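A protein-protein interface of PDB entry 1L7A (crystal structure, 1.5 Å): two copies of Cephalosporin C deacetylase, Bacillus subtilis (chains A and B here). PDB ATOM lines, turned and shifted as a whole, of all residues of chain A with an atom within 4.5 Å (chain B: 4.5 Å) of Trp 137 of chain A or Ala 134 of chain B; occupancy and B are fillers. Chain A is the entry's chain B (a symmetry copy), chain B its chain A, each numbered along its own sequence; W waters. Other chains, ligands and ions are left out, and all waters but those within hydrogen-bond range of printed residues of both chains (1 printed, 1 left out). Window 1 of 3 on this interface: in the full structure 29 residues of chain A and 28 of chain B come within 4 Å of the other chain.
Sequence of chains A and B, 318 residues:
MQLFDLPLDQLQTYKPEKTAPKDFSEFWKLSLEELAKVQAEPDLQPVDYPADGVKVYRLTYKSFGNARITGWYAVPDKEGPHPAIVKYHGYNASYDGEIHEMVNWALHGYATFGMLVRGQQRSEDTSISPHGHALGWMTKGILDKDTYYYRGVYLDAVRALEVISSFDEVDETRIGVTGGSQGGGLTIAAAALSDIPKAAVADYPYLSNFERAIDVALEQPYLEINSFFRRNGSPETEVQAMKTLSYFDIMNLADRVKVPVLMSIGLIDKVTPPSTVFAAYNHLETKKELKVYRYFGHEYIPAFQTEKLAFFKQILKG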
ATOM      1  N   TYR A  91      10.676  24.938  36.330  1.00  0.00           N
ATOM      2  CA  TYR A  91      10.397  25.371  34.958  1.00  0.00           C
ATOM      3  C   TYR A  91       9.412  26.529  34.899  1.00  0.00           C
ATOM      4  O   TYR A  91       8.267  26.395  35.340  1.00  0.00           O
ATOM      5  CB  TYR A  91       9.845  24.188  34.178  1.00  0.00           C
ATOM      6  CG  TYR A  91       9.606  24.368  32.707  1.00  0.00           C
ATOM      7  CD1 TYR A  91       8.370  24.746  32.195  1.00  0.00           C
ATOM      8  CD2 TYR A  91      10.636  24.150  31.804  1.00  0.00           C
ATOM      9  CE1 TYR A  91       8.180  24.903  30.839  1.00  0.00           C
ATOM     10  CE2 TYR A  91      10.455  24.314  30.442  1.00  0.00           C
ATOM     11  CZ  TYR A  91       9.212  24.676  29.968  1.00  0.00           C
ATOM     12  OH  TYR A  91       9.030  24.828  28.621  1.00  0.00           O
ATOM     13  N   ASN A  92       9.833  27.679  34.384  1.00  0.00           N
ATOM     14  CA  ASN A  92       8.981  28.852  34.280  1.00  0.00           C
ATOM     15  C   ASN A  92       8.421  29.224  35.642  1.00  0.00           C
ATOM     16  O   ASN A  92       7.418  29.925  35.718  1.00  0.00           O
ATOM     17  CB  ASN A  92       7.778  28.573  33.369  1.00  0.00           C
ATOM     18  CG  ASN A  92       6.973  29.796  32.970  1.00  0.00           C
ATOM     19  OD1 ASN A  92       7.556  30.801  32.550  1.00  0.00           O
ATOM     20  ND2 ASN A  92       5.653  29.705  33.032  1.00  0.00           N
ATOM     21  N   GLY A 119      16.931  32.385  29.707  1.00  0.00           N
ATOM     22  CA  GLY A 119      15.695  32.463  28.940  1.00  0.00           C
ATOM     23  C   GLY A 119      14.437  32.469  29.804  1.00  0.00           C
ATOM     24  O   GLY A 119      13.419  32.891  29.249  1.00  0.00           O
ATOM     25  N   GLN A 120      14.488  31.944  31.016  1.00  0.00           N
ATOM     26  CA  GLN A 120      13.302  31.894  31.854  1.00  0.00           C
ATOM     27  C   GLN A 120      13.163  33.041  32.840  1.00  0.00           C
ATOM     28  O   GLN A 120      12.069  33.568  33.052  1.00  0.00           O
ATOM     29  CB  GLN A 120      13.232  30.603  32.675  1.00  0.00           C
ATOM     30  CG  GLN A 120      13.106  29.364  31.807  1.00  0.00           C
ATOM     31  CD  GLN A 120      13.082  28.072  32.589  1.00  0.00           C
ATOM     32  OE1 GLN A 120      12.663  27.912  33.744  1.00  0.00           O
ATOM     33  NE2 GLN A 120      13.530  27.024  31.895  1.00  0.00           N
ATOM     34  N   GLY A 136       7.081  26.978  24.549  1.00  0.00           N
ATOM     35  CA  GLY A 136       7.900  26.589  25.692  1.00  0.00           C
ATOM     36  C   GLY A 136       9.358  26.413  25.290  1.00  0.00           C
ATOM     37  O   GLY A 136       9.768  26.744  24.175  1.00  0.00           O
ATOM     38  N   TRP A 137      10.160  25.919  26.233  1.00  0.00           N
ATOM     39  CA  TRP A 137      11.576  25.671  26.012  1.00  0.00           C
ATOM     40  C   TRP A 137      11.921  24.194  25.827  1.00  0.00           C
ATOM     41  O   TRP A 137      13.033  23.910  25.378  1.00  0.00           O
ATOM     42  CB  TRP A 137      12.399  26.199  27.199  1.00  0.00           C
ATOM     43  CG  TRP A 137      12.365  27.680  27.444  1.00  0.00           C
ATOM     44  CD1 TRP A 137      13.180  28.633  26.888  1.00  0.00           C
ATOM     45  CD2 TRP A 137      11.489  28.385  28.334  1.00  0.00           C
ATOM     46  NE1 TRP A 137      12.866  29.875  27.390  1.00  0.00           N
ATOM     47  CE2 TRP A 137      11.819  29.751  28.258  1.00  0.00           C
ATOM     48  CE3 TRP A 137      10.431  27.991  29.155  1.00  0.00           C
ATOM     49  CZ2 TRP A 137      11.138  30.723  28.996  1.00  0.00           C
ATOM     50  CZ3 TRP A 137       9.794  28.959  29.917  1.00  0.00           C
ATOM     51  CH2 TRP A 137      10.117  30.319  29.805  1.00  0.00           C
ATOM     52  N   MET A 138      10.999  23.279  26.117  1.00  0.00           N
ATOM     53  CA  MET A 138      11.327  21.862  26.067  1.00  0.00           C
ATOM     54  C   MET A 138      11.747  21.344  24.714  1.00  0.00           C
ATOM     55  O   MET A 138      12.450  20.331  24.697  1.00  0.00           O
ATOM     56  CB  MET A 138      10.141  21.005  26.505  1.00  0.00           C
ATOM     57  CG  MET A 138       9.767  21.210  27.964  1.00  0.00           C
ATOM     58  SD  MET A 138      11.079  20.850  29.215  1.00  0.00           S
ATOM     59  CE  MET A 138      11.394  19.107  28.865  1.00  0.00           C
ATOM     60  N   THR A 139      11.278  21.948  23.629  1.00  0.00           N
ATOM     61  CA  THR A 139      11.633  21.456  22.302  1.00  0.00           C
ATOM     62  C   THR A 139      12.542  22.387  21.528  1.00  0.00           C
ATOM     63  O   THR A 139      12.766  22.176  20.326  1.00  0.00           O
ATOM     64  CB  THR A 139      10.352  21.043  21.536  1.00  0.00           C
ATOM     65  OG1 THR A 139       9.411  22.116  21.385  1.00  0.00           O
ATOM     66  CG2 THR A 139       9.697  19.904  22.309  1.00  0.00           C
ATOM     67  N   LYS A 140      12.991  23.479  22.148  1.00  0.00           N
ATOM     68  CA  LYS A 140      13.884  24.432  21.504  1.00  0.00           C
ATOM     69  C   LYS A 140      15.221  23.749  21.181  1.00  0.00           C
ATOM     70  O   LYS A 140      15.933  23.304  22.095  1.00  0.00           O
ATOM     71  CB  LYS A 140      14.053  25.661  22.411  1.00  0.00           C
ATOM     72  CG  LYS A 140      15.025  26.701  21.876  1.00  0.00           C
ATOM     73  CD  LYS A 140      14.922  27.968  22.729  1.00  0.00           C
ATOM     74  CE  LYS A 140      15.841  29.062  22.218  1.00  0.00           C
ATOM     75  NZ  LYS A 140      17.270  28.737  22.541  1.00  0.00           N
ATOM     76  N   TYR A 149      18.131  23.170  24.054  1.00  0.00           N
ATOM     77  CA  TYR A 149      18.048  24.108  25.165  1.00  0.00           C
ATOM     78  C   TYR A 149      18.764  23.711  26.437  1.00  0.00           C
ATOM     79  O   TYR A 149      19.486  24.558  26.983  1.00  0.00           O
ATOM     80  CB  TYR A 149      16.555  24.293  25.486  1.00  0.00           C
ATOM     81  CG  TYR A 149      16.291  25.235  26.636  1.00  0.00           C
ATOM     82  CD1 TYR A 149      16.589  26.587  26.544  1.00  0.00           C
ATOM     83  CD2 TYR A 149      15.719  24.763  27.805  1.00  0.00           C
ATOM     84  CE1 TYR A 149      16.323  27.451  27.598  1.00  0.00           C
ATOM     85  CE2 TYR A 149      15.455  25.617  28.876  1.00  0.00           C
ATOM     86  CZ  TYR A 149      15.755  26.947  28.739  1.00  0.00           C
ATOM     87  OH  TYR A 149      15.475  27.785  29.795  1.00  0.00           O
ATOM     88  N   GLU A 224       4.959  19.222  26.305  1.00  0.00           N
ATOM     89  CA  GLU A 224       5.408  20.080  25.211  1.00  0.00           C
ATOM     90  C   GLU A 224       6.049  19.216  24.123  1.00  0.00           C
ATOM     91  O   GLU A 224       6.011  19.586  22.942  1.00  0.00           O
ATOM     92  CB  GLU A 224       6.453  21.093  25.664  1.00  0.00           C
ATOM     93  CG  GLU A 224       5.904  22.172  26.576  1.00  0.00           C
ATOM     94  CD  GLU A 224       6.943  23.211  26.941  1.00  0.00           C
ATOM     95  OE1 GLU A 224       7.984  23.313  26.252  1.00  0.00           O
ATOM     96  OE2 GLU A 224       6.699  23.946  27.937  1.00  0.00           O
ATOM     97  N   HIS B 133      12.143  35.439  29.988  1.00  0.00           N
ATOM     98  CA  HIS B 133      10.759  35.786  29.684  1.00  0.00           C
ATOM     99  C   HIS B 133       9.811  34.698  30.154  1.00  0.00           C
ATOM    100  O   HIS B 133      10.237  33.597  30.473  1.00  0.00           O
ATOM    101  CB  HIS B 133      10.610  35.965  28.160  1.00  0.00           C
ATOM    102  CG  HIS B 133      10.982  34.798  27.301  1.00  0.00           C
ATOM    103  ND1 HIS B 133      10.108  33.756  27.066  1.00  0.00           N
ATOM    104  CD2 HIS B 133      12.132  34.481  26.641  1.00  0.00           C
ATOM    105  CE1 HIS B 133      10.693  32.863  26.286  1.00  0.00           C
ATOM    106  NE2 HIS B 133      11.908  33.277  26.012  1.00  0.00           N
ATOM    107  N   ALA B 134       8.529  35.058  30.250  1.00  0.00           N
ATOM    108  CA  ALA B 134       7.537  34.050  30.625  1.00  0.00           C
ATOM    109  C   ALA B 134       7.389  33.043  29.490  1.00  0.00           C
ATOM    110  O   ALA B 134       7.636  33.302  28.313  1.00  0.00           O
ATOM    111  CB  ALA B 134       6.203  34.742  30.846  1.00  0.00           C
ATOM    112  N   LEU B 135       6.905  31.857  29.801  1.00  0.00           N
ATOM    113  CA  LEU B 135       6.675  30.773  28.863  1.00  0.00           C
ATOM    114  C   LEU B 135       5.954  31.350  27.646  1.00  0.00           C
ATOM    115  O   LEU B 135       4.870  31.930  27.751  1.00  0.00           O
ATOM    116  CB  LEU B 135       5.845  29.664  29.523  1.00  0.00           C
ATOM    117  CG  LEU B 135       5.908  28.343  28.722  1.00  0.00           C
ATOM    118  CD1 LEU B 135       5.716  27.205  29.711  1.00  0.00           C
ATOM    119  CD2 LEU B 135       4.924  28.344  27.567  1.00  0.00           C
ATOM    120  N   GLY B 136       6.543  31.081  26.482  1.00  0.00           N
ATOM    121  CA  GLY B 136       5.992  31.576  25.224  1.00  0.00           C
ATOM    122  C   GLY B 136       6.928  32.583  24.573  1.00  0.00           C
ATOM    123  O   GLY B 136       8.087  32.759  24.986  1.00  0.00           O
ATOM    124  N   THR B 139       6.817  37.624  25.417  1.00  0.00           N
ATOM    125  CA  THR B 139       7.645  38.512  26.229  1.00  0.00           C
ATOM    126  C   THR B 139       9.127  38.378  25.939  1.00  0.00           C
ATOM    127  O   THR B 139       9.928  38.984  26.648  1.00  0.00           O
ATOM    128  CB  THR B 139       7.264  38.375  27.721  1.00  0.00           C
ATOM    129  OG1 THR B 139       7.435  37.052  28.212  1.00  0.00           O
ATOM    130  CG2 THR B 139       5.805  38.800  27.894  1.00  0.00           C
ATOM    131  N   GLU B 224       0.272  35.993  28.502  1.00  0.00           N
ATOM    132  CA  GLU B 224       1.679  35.758  28.749  1.00  0.00           C
ATOM    133  C   GLU B 224       2.275  37.058  29.282  1.00  0.00           C
ATOM    134  O   GLU B 224       3.285  37.044  29.985  1.00  0.00           O
ATOM    135  CB  GLU B 224       2.446  35.345  27.483  1.00  0.00           C
ATOM    136  CG  GLU B 224       2.031  33.986  26.946  1.00  0.00           C
ATOM    137  CD  GLU B 224       2.920  33.612  25.782  1.00  0.00           C
ATOM    138  OE1 GLU B 224       3.974  34.232  25.522  1.00  0.00           O
ATOM    139  OE2 GLU B 224       2.500  32.658  25.091  1.00  0.00           O
ATOM    140  N   SER B 227       1.642  37.184  32.828  1.00  0.00           N
ATOM    141  CA  SER B 227       2.529  36.192  33.442  1.00  0.00           C
ATOM    142  C   SER B 227       3.930  36.736  33.634  1.00  0.00           C
ATOM    143  O   SER B 227       4.605  36.406  34.616  1.00  0.00           O
ATOM    144  CB  SER B 227       2.546  34.937  32.586  1.00  0.00           C
ATOM    145  OG  SER B 227       1.271  34.322  32.668  1.00  0.00           O
ATOM    146  N   PHE B 228       4.447  37.472  32.653  1.00  0.00           N
ATOM    147  CA  PHE B 228       5.766  38.072  32.747  1.00  0.00           C
ATOM    148  C   PHE B 228       5.794  39.100  33.857  1.00  0.00           C
ATOM    149  O   PHE B 228       6.790  39.145  34.593  1.00  0.00           O
ATOM    150  CB  PHE B 228       6.111  38.684  31.404  1.00  0.00           C
ATOM    151  CG  PHE B 228       7.411  39.445  31.367  1.00  0.00           C
ATOM    152  CD1 PHE B 228       8.622  38.761  31.324  1.00  0.00           C
ATOM    153  CD2 PHE B 228       7.413  40.819  31.372  1.00  0.00           C
ATOM    154  CE1 PHE B 228       9.808  39.478  31.260  1.00  0.00           C
ATOM    155  CE2 PHE B 228       8.598  41.532  31.301  1.00  0.00           C
ATOM    156  CZ  PHE B 228       9.799  40.854  31.260  1.00  0.00           C
ATOM    157  N   ARG B 231       6.234  37.470  37.161  1.00  0.00           N
ATOM    158  CA  ARG B 231       7.582  36.964  37.418  1.00  0.00           C
ATOM    159  C   ARG B 231       8.680  38.009  37.447  1.00  0.00           C
ATOM    160  O   ARG B 231       9.790  37.718  37.882  1.00  0.00           O
ATOM    161  CB  ARG B 231       7.881  35.927  36.323  1.00  0.00           C
ATOM    162  CG  ARG B 231       7.107  34.626  36.425  1.00  0.00           C
ATOM    163  CD  ARG B 231       6.990  33.892  35.090  1.00  0.00           C
ATOM    164  NE  ARG B 231       6.364  32.601  35.336  1.00  0.00           N
ATOM    165  CZ  ARG B 231       5.084  32.398  35.591  1.00  0.00           C
ATOM    166  NH1 ARG B 231       4.249  33.437  35.612  1.00  0.00           N
ATOM    167  NH2 ARG B 231       4.632  31.182  35.824  1.00  0.00           N
HETATM  168  O   HOH W   1      10.757  36.029  33.006  1.00  0.00           O
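Of the 9 printed residues of chain B, 4 touch a printed residue of chain A.
Printed residues of chain B that touch a printed residue of chain A: His 133, Ala 134, Leu 135 and Arg 231.
Among the printed residues, 11 pairs touch across the chains.
OE1 of Gln 120 of chain A is in hydrogen-bond range of N of Asn 92 of chain A (2.9 Å).
The side-chain hydroxyl of Tyr 91 of chain A is in hydrogen-bond range of the backbone NH of Trp 137 of chain A.
The side-chain carboxylate (OE1) of Glu 224 of chain A lies within hydrogen-bond range of the backbone NH (N) of Trp 137 of chain A (3.4 Å).
The backbone NH (N) of Ala 134 of chain B sits at hydrogen-bond distance from the side-chain hydroxyl (OG1) of Thr 139 of chain B (3.1 Å).
OH of Tyr 149 of chain A lies within hydrogen-bond range of NE2 of Gln 120 of chain A (3.0 Å).
The side-chain hydroxyl (OH) of Tyr 91 of chain A sits at hydrogen-bond distance from the side-chain carboxylate (OE2) of Glu 224 of chain A.
The backbone carbonyl oxygen (O) of Asn 92 of chain A lies within hydrogen-bond range of the guanidinium group (NE) of Arg 231 of chain B.
The backbone carbonyl oxygen of Gln 120 of chain A sits close to the backbone carbonyl oxygen of His 133 of chain B, at 3.2 Å.
N of Leu 135 of chain B lies within hydrogen-bond range of OD1 of Asn 92 of chain A (3.0 Å).
N of His 133 of chain B lies within hydrogen-bond range of O of Gly 119 of chain A, at 2.9 Å.
3 positions are printed for both chains.
Of the 11 pairs that touch across the chains among the printed residues, none has its exchanged pair printed and touching as well.
Tyr 91 of chain A touches Leu 135 of chain B (CE1 to CD1, 3.6 Å).
Asn 92 of chain A touches Ala 134 of chain B.
Leu 135 of chain B touches Gly 136 of chain A.
His 133 of chain B touches Trp 137 of chain A.
CH2 of Trp 137 of chain A touches C of Ala 134 of chain B, 3.9 Å away.
Leu 135 of chain B touches Trp 137 of chain A.
OE2 of Glu 224 of chain A touches CD1 of Leu 135 of chain B (3.8 Å).
Water W1 lies within hydrogen-bond range of O of Gln 120 of chain A (2.8 Å) and N of His 133 of chain B (3.4 Å).
Of the printed residues of chain B, Asn 92 of chain A touches Ala 134, Leu 135 and Arg 231.
Of the printed residues of chain B, Gly 136 of chain A touches Leu 135.
Of the printed residues of chain B, Trp 137 of chain A touches His 133, Ala 134 and Leu 135.
Ala 134 of chain B touches just these residues of chain A: Asn 92 (3.8 Å) and Trp 137 (3.9 Å).
The nearest printed residue of chain A that does not touch Ala 134 of chain B is Gln 120 of chain A (4.8 Å).
The nearest printed residue of chain B that does not touch Gly 119 of chain A is Ala 134 of chain B (5.4 Å).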
